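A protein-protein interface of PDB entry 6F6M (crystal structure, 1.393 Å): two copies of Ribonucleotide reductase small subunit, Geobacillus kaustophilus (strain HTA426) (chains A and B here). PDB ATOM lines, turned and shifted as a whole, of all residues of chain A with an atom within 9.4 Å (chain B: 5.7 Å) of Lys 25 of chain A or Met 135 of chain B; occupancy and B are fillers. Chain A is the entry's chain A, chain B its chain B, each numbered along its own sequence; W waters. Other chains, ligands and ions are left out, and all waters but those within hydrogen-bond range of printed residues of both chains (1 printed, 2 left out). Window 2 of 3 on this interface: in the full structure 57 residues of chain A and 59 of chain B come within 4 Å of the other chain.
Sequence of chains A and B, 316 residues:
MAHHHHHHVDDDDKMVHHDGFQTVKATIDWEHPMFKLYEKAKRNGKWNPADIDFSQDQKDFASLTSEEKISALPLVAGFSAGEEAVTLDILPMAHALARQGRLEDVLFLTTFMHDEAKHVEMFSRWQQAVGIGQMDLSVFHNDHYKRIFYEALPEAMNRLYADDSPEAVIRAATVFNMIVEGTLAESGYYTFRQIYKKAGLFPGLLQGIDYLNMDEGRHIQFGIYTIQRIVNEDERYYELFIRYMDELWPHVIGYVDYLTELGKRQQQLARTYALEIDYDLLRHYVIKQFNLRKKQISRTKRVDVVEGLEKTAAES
O of Val 24 of chain A sits at hydrogen-bond distance from N of Leu 137 of chain B (2.9 Å).
The backbone carbonyl oxygen of Ala 26 of chain A lies close to the backbone carbonyl oxygen of Gly 133 of chain B (3.4 Å).
O of Met 135 of chain B lies close to O of Val 24 of chain A, 3.3 Å away.
The side-chain amide oxygen (OE1) of Gln 127 of chain B lies close to the backbone carbonyl oxygen (O) of Thr 23 of chain A (2.9 Å).
O of Gln 127 of chain B sits at hydrogen-bond distance from N of Gly 133 of chain B.
The backbone carbonyl oxygen (O) of Gln 127 of chain B is in hydrogen-bond range of the backbone NH (N) of Ile 132 of chain B, 3.0 Å away.
The side-chain carboxylate (OD1) of Asp 136 of chain B sits at hydrogen-bond distance from the side-chain hydroxyl (OG) of Ser 138 of chain B (2.7 Å).
O of Thr 27 of chain A lies within hydrogen-bond range of NE2 of Gln 22 of chain A, at 3.0 Å.
Among the printed residues, pairs that only touch across the chains: Val 24 of chain A with Asp 136 of chain B, Val 24 of chain A with Ser 138 of chain B, Lys 25 of chain A with Met 135 of chain B, Lys 25 of chain A with Asp 136 of chain B, Lys 25 of chain A with Ser 138 of chain B and Thr 27 of chain A with Gly 133 of chain B.
Of the printed residues of chain B, Thr 23 of chain A touches Gln 127.
Printed residues of chain B within 4 Å of Val 24 of chain A: Met 135 (3.3 Å), Asp 136 (3.7 Å), Leu 137 (2.9 Å) and Ser 138 (3.2 Å).
Of chain B, only Met 135, Asp 136 and Ser 138 come within 4 Å of Lys 25 of chain A.
Ile 28 of chain A touches none of the printed residues of chain B.
Gly 133 of chain B touches just these residues of chain A: Ala 26 and Thr 27.
No residue of chain A comes within 4 Å of Gln 134 of chain B.
Met 135 of chain B touches just these residues of chain A: Val 24 and Lys 25.
Printed residues of chain A within 4 Å of Ser 138 of chain B: Val 24 and Lys 25.
The nearest printed residue of chain A that does not touch Leu 137 of chain B is Lys 25 of chain A (4.7 Å).
Of the 10 printed residues of chain B, 6 touch a printed residue of chain A.
Hydrophobic or aromatic side chains of chain A within 4 Å of the printed part of chain B: Val 24.
No position is printed for both chains.
Water W1 bridges OG of Ser 138 of chain B (2.9 Å) and N of Phe 21 of chain A (3.1 Å).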
ATOM      1  N   HIS A  18       7.096 -31.794  -7.833  1.00  0.00           N
ATOM      2  CA  HIS A  18       7.781 -30.745  -7.093  1.00  0.00           C
ATOM      3  C   HIS A  18       7.795 -31.104  -5.617  1.00  0.00           C
ATOM      4  O   HIS A  18       6.749 -31.425  -5.044  1.00  0.00           O
ATOM      5  CB  HIS A  18       7.075 -29.406  -7.274  1.00  0.00           C
ATOM      6  CG  HIS A  18       7.091 -28.895  -8.679  1.00  0.00           C
ATOM      7  ND1 HIS A  18       8.256 -28.555  -9.338  1.00  0.00           N
ATOM      8  CD2 HIS A  18       6.081 -28.635  -9.544  1.00  0.00           C
ATOM      9  CE1 HIS A  18       7.960 -28.117 -10.549  1.00  0.00           C
ATOM     10  NE2 HIS A  18       6.648 -28.172 -10.704  1.00  0.00           N
ATOM     11  N   ASP A  19       8.981 -31.039  -5.009  1.00  0.00           N
ATOM     12  CA  ASP A  19       9.139 -31.368  -3.595  1.00  0.00           C
ATOM     13  C   ASP A  19       8.631 -30.235  -2.719  1.00  0.00           C
ATOM     14  O   ASP A  19       8.022 -30.461  -1.667  1.00  0.00           O
ATOM     15  CB  ASP A  19      10.622 -31.600  -3.305  1.00  0.00           C
ATOM     16  CG  ASP A  19      10.907 -31.749  -1.827  1.00  0.00           C
ATOM     17  OD1 ASP A  19       9.974 -32.118  -1.079  1.00  0.00           O
ATOM     18  OD2 ASP A  19      12.061 -31.494  -1.412  1.00  0.00           O
ATOM     19  N   GLY A  20       8.911 -29.020  -3.150  1.00  0.00           N
ATOM     20  CA  GLY A  20       8.423 -27.805  -2.544  1.00  0.00           C
ATOM     21  C   GLY A  20       8.826 -26.696  -3.478  1.00  0.00           C
ATOM     22  O   GLY A  20       9.282 -26.958  -4.592  1.00  0.00           O
ATOM     23  N   PHE A  21       8.695 -25.456  -3.006  1.00  0.00           N
ATOM     24  CA  PHE A  21       8.987 -24.294  -3.831  1.00  0.00           C
ATOM     25  C   PHE A  21       9.832 -23.308  -3.030  1.00  0.00           C
ATOM     26  O   PHE A  21       9.519 -23.002  -1.873  1.00  0.00           O
ATOM     27  CB  PHE A  21       7.689 -23.659  -4.322  1.00  0.00           C
ATOM     28  CG  PHE A  21       6.907 -24.555  -5.229  1.00  0.00           C
ATOM     29  CD1 PHE A  21       7.269 -24.709  -6.559  1.00  0.00           C
ATOM     30  CD2 PHE A  21       5.821 -25.271  -4.741  1.00  0.00           C
ATOM     31  CE1 PHE A  21       6.546 -25.563  -7.400  1.00  0.00           C
ATOM     32  CE2 PHE A  21       5.101 -26.116  -5.570  1.00  0.00           C
ATOM     33  CZ  PHE A  21       5.452 -26.265  -6.889  1.00  0.00           C
ATOM     34  N   GLN A  22      10.913 -22.835  -3.650  1.00  0.00           N
ATOM     35  CA  GLN A  22      11.860 -21.957  -2.971  1.00  0.00           C
ATOM     36  C   GLN A  22      11.201 -20.661  -2.511  1.00  0.00           C
ATOM     37  O   GLN A  22      11.533 -20.142  -1.437  1.00  0.00           O
ATOM     38  CB  GLN A  22      13.013 -21.643  -3.921  1.00  0.00           C
ATOM     39  CG  GLN A  22      14.110 -20.777  -3.311  1.00  0.00           C
ATOM     40  CD  GLN A  22      15.214 -20.489  -4.299  1.00  0.00           C
ATOM     41  OE1 GLN A  22      15.611 -21.351  -5.092  1.00  0.00           O
ATOM     42  NE2 GLN A  22      15.722 -19.259  -4.268  1.00  0.00           N
ATOM     43  N   THR A  23      10.281 -20.107  -3.308  1.00  0.00           N
ATOM     44  CA  THR A  23       9.657 -18.838  -2.922  1.00  0.00           C
ATOM     45  C   THR A  23       8.463 -19.013  -1.978  1.00  0.00           C
ATOM     46  O   THR A  23       7.802 -18.022  -1.631  1.00  0.00           O
ATOM     47  CB  THR A  23       9.287 -17.988  -4.148  1.00  0.00           C
ATOM     48  OG1 THR A  23       8.311 -18.658  -4.949  1.00  0.00           O
ATOM     49  CG2 THR A  23      10.516 -17.714  -5.010  1.00  0.00           C
ATOM     50  N   VAL A  24       8.170 -20.244  -1.555  1.00  0.00           N
ATOM     51  CA  VAL A  24       7.255 -20.490  -0.443  1.00  0.00           C
ATOM     52  C   VAL A  24       8.014 -20.791   0.844  1.00  0.00           C
ATOM     53  O   VAL A  24       7.665 -20.287   1.916  1.00  0.00           O
ATOM     54  CB  VAL A  24       6.296 -21.644  -0.810  1.00  0.00           C
ATOM     55  CG1 VAL A  24       5.425 -22.049   0.358  1.00  0.00           C
ATOM     56  CG2 VAL A  24       5.421 -21.240  -1.940  1.00  0.00           C
ATOM     57  N   LYS A  25       9.062 -21.612   0.748  1.00  0.00           N
ATOM     58  CA  LYS A  25       9.872 -21.928   1.914  1.00  0.00           C
ATOM     59  C   LYS A  25      10.768 -20.751   2.306  1.00  0.00           C
ATOM     60  O   LYS A  25      11.103 -20.587   3.485  1.00  0.00           O
ATOM     61  CB  LYS A  25      10.690 -23.176   1.608  1.00  0.00           C
ATOM     62  CG  LYS A  25       9.789 -24.400   1.420  1.00  0.00           C
ATOM     63  CD  LYS A  25      10.358 -25.421   0.428  1.00  0.00           C
ATOM     64  CE  LYS A  25      11.569 -26.140   0.974  1.00  0.00           C
ATOM     65  NZ  LYS A  25      12.101 -27.167   0.015  1.00  0.00           N
ATOM     66  N   ALA A  26      11.155 -19.925   1.336  1.00  0.00           N
ATOM     67  CA  ALA A  26      12.093 -18.838   1.582  1.00  0.00           C
ATOM     68  C   ALA A  26      11.827 -17.744   0.562  1.00  0.00           C
ATOM     69  O   ALA A  26      10.673 -17.383   0.370  1.00  0.00           O
ATOM     70  CB  ALA A  26      13.530 -19.362   1.516  1.00  0.00           C
ATOM     71  N   THR A  27      12.867 -17.234  -0.118  1.00  0.00           N
ATOM     72  CA  THR A  27      12.705 -16.254  -1.180  1.00  0.00           C
ATOM     73  C   THR A  27      13.721 -16.573  -2.266  1.00  0.00           C
ATOM     74  O   THR A  27      14.555 -17.476  -2.132  1.00  0.00           O
ATOM     75  CB  THR A  27      12.987 -14.819  -0.712  1.00  0.00           C
ATOM     76  OG1 THR A  27      14.375 -14.695  -0.387  1.00  0.00           O
ATOM     77  CG2 THR A  27      12.134 -14.439   0.507  1.00  0.00           C
ATOM     78  N   ILE A  28      13.649 -15.806  -3.346  1.00  0.00           N
ATOM     79  CA  ILE A  28      14.722 -15.733  -4.319  1.00  0.00           C
ATOM     80  C   ILE A  28      16.024 -15.398  -3.599  1.00  0.00           C
ATOM     81  O   ILE A  28      16.037 -14.638  -2.615  1.00  0.00           O
ATOM     82  CB  ILE A  28      14.382 -14.664  -5.371  1.00  0.00           C
ATOM     83  CG1 ILE A  28      13.181 -15.115  -6.216  1.00  0.00           C
ATOM     84  CG2 ILE A  28      15.586 -14.373  -6.263  1.00  0.00           C
ATOM     85  CD1 ILE A  28      12.702 -14.108  -7.217  1.00  0.00           C
ATOM     86  N   LEU B  73      -1.952 -14.713   4.125  1.00  0.00           N
ATOM     87  CA  LEU B  73      -0.839 -15.582   3.760  1.00  0.00           C
ATOM     88  C   LEU B  73      -1.251 -16.816   2.963  1.00  0.00           C
ATOM     89  O   LEU B  73      -0.473 -17.260   2.107  1.00  0.00           O
ATOM     90  CB  LEU B  73      -0.044 -15.979   5.002  1.00  0.00           C
ATOM     91  CG  LEU B  73       0.611 -14.814   5.756  1.00  0.00           C
ATOM     92  CD1 LEU B  73       1.544 -15.357   6.800  1.00  0.00           C
ATOM     93  CD2 LEU B  73       1.351 -13.842   4.821  1.00  0.00           C
ATOM     94  N   GLN B 127       6.891 -10.752  -0.277  1.00  0.00           N
ATOM     95  CA  GLN B 127       7.177 -11.474   0.953  1.00  0.00           C
ATOM     96  C   GLN B 127       8.402 -10.914   1.648  1.00  0.00           C
ATOM     97  O   GLN B 127       8.405 -10.721   2.869  1.00  0.00           O
ATOM     98  CB  GLN B 127       7.394 -12.943   0.635  1.00  0.00           C
ATOM     99  CG  GLN B 127       6.144 -13.675   0.187  1.00  0.00           C
ATOM    100  CD  GLN B 127       6.376 -15.173   0.151  1.00  0.00           C
ATOM    101  OE1 GLN B 127       5.989 -15.881  -0.801  1.00  0.00           O
ATOM    102  NE2 GLN B 127       7.016 -15.679   1.192  1.00  0.00           N
ATOM    103  N   GLY B 131       8.379  -8.746   5.421  1.00  0.00           N
ATOM    104  CA  GLY B 131       9.038  -9.390   6.532  1.00  0.00           C
ATOM    105  C   GLY B 131       8.647 -10.825   6.785  1.00  0.00           C
ATOM    106  O   GLY B 131       8.832 -11.299   7.908  1.00  0.00           O
ATOM    107  N   ILE B 132       8.168 -11.542   5.766  1.00  0.00           N
ATOM    108  CA  ILE B 132       7.807 -12.949   5.886  1.00  0.00           C
ATOM    109  C   ILE B 132       8.636 -13.836   4.974  1.00  0.00           C
ATOM    110  O   ILE B 132       8.325 -15.023   4.804  1.00  0.00           O
ATOM    111  CB  ILE B 132       6.294 -13.182   5.686  1.00  0.00           C
ATOM    112  CG1 ILE B 132       5.878 -12.938   4.223  1.00  0.00           C
ATOM    113  CG2 ILE B 132       5.514 -12.315   6.655  1.00  0.00           C
ATOM    114  CD1 ILE B 132       4.446 -13.318   3.930  1.00  0.00           C
ATOM    115  N   GLY B 133       9.684 -13.291   4.362  1.00  0.00           N
ATOM    116  CA  GLY B 133      10.513 -14.099   3.487  1.00  0.00           C
ATOM    117  C   GLY B 133      11.032 -15.332   4.176  1.00  0.00           C
ATOM    118  O   GLY B 133      11.159 -16.398   3.548  1.00  0.00           O
ATOM    119  N   GLN B 134      11.304 -15.219   5.477  1.00  0.00           N
ATOM    120  CA  GLN B 134      11.882 -16.287   6.276  1.00  0.00           C
ATOM    121  C   GLN B 134      10.843 -17.294   6.769  1.00  0.00           C
ATOM    122  O   GLN B 134      11.230 -18.317   7.326  1.00  0.00           O
ATOM    123  CB  GLN B 134      12.669 -15.694   7.466  1.00  0.00           C
ATOM    124  CG  GLN B 134      11.839 -15.110   8.602  1.00  0.00           C
ATOM    125  CD  GLN B 134      11.047 -13.862   8.248  1.00  0.00           C
ATOM    126  OE1 GLN B 134      11.368 -13.145   7.296  1.00  0.00           O
ATOM    127  NE2 GLN B 134      10.016 -13.575   9.036  1.00  0.00           N
ATOM    128  N   MET B 135       9.550 -17.044   6.544  1.00  0.00           N
ATOM    129  CA  MET B 135       8.484 -17.917   7.020  1.00  0.00           C
ATOM    130  C   MET B 135       8.149 -18.958   5.955  1.00  0.00           C
ATOM    131  O   MET B 135       7.990 -18.621   4.783  1.00  0.00           O
ATOM    132  CB  MET B 135       7.255 -17.058   7.314  1.00  0.00           C
ATOM    133  CG  MET B 135       6.097 -17.780   7.963  1.00  0.00           C
ATOM    134  SD  MET B 135       4.632 -16.724   8.042  1.00  0.00           S
ATOM    135  CE  MET B 135       5.335 -15.188   8.678  1.00  0.00           C
ATOM    136  N   ASP B 136       8.042 -20.222   6.362  1.00  0.00           N
ATOM    137  CA  ASP B 136       7.720 -21.303   5.423  1.00  0.00           C
ATOM    138  C   ASP B 136       6.211 -21.345   5.223  1.00  0.00           C
ATOM    139  O   ASP B 136       5.472 -21.784   6.111  1.00  0.00           O
ATOM    140  CB  ASP B 136       8.241 -22.639   5.936  1.00  0.00           C
ATOM    141  CG  ASP B 136       7.989 -23.789   4.951  1.00  0.00           C
ATOM    142  OD1 ASP B 136       7.333 -23.561   3.899  1.00  0.00           O
ATOM    143  OD2 ASP B 136       8.453 -24.916   5.232  1.00  0.00           O
ATOM    144  N   LEU B 137       5.746 -20.905   4.056  1.00  0.00           N
ATOM    145  CA  LEU B 137       4.317 -20.789   3.796  1.00  0.00           C
ATOM    146  C   LEU B 137       3.706 -22.069   3.243  1.00  0.00           C
ATOM    147  O   LEU B 137       2.534 -22.053   2.850  1.00  0.00           O
ATOM    148  CB  LEU B 137       4.042 -19.614   2.853  1.00  0.00           C
ATOM    149  CG  LEU B 137       4.435 -18.228   3.366  1.00  0.00           C
ATOM    150  CD1 LEU B 137       4.114 -17.181   2.310  1.00  0.00           C
ATOM    151  CD2 LEU B 137       3.743 -17.911   4.676  1.00  0.00           C
ATOM    152  N   SER B 138       4.476 -23.166   3.203  1.00  0.00           N
ATOM    153  CA  SER B 138       3.994 -24.443   2.692  1.00  0.00           C
ATOM    154  C   SER B 138       2.839 -24.971   3.513  1.00  0.00           C
ATOM    155  O   SER B 138       2.082 -25.828   3.042  1.00  0.00           O
ATOM    156  CB  SER B 138       5.110 -25.492   2.782  1.00  0.00           C
ATOM    157  OG  SER B 138       6.214 -25.131   1.970  1.00  0.00           O
HETATM  158  O   HOH W   1       6.498 -25.365  -0.874  1.00  0.00           O
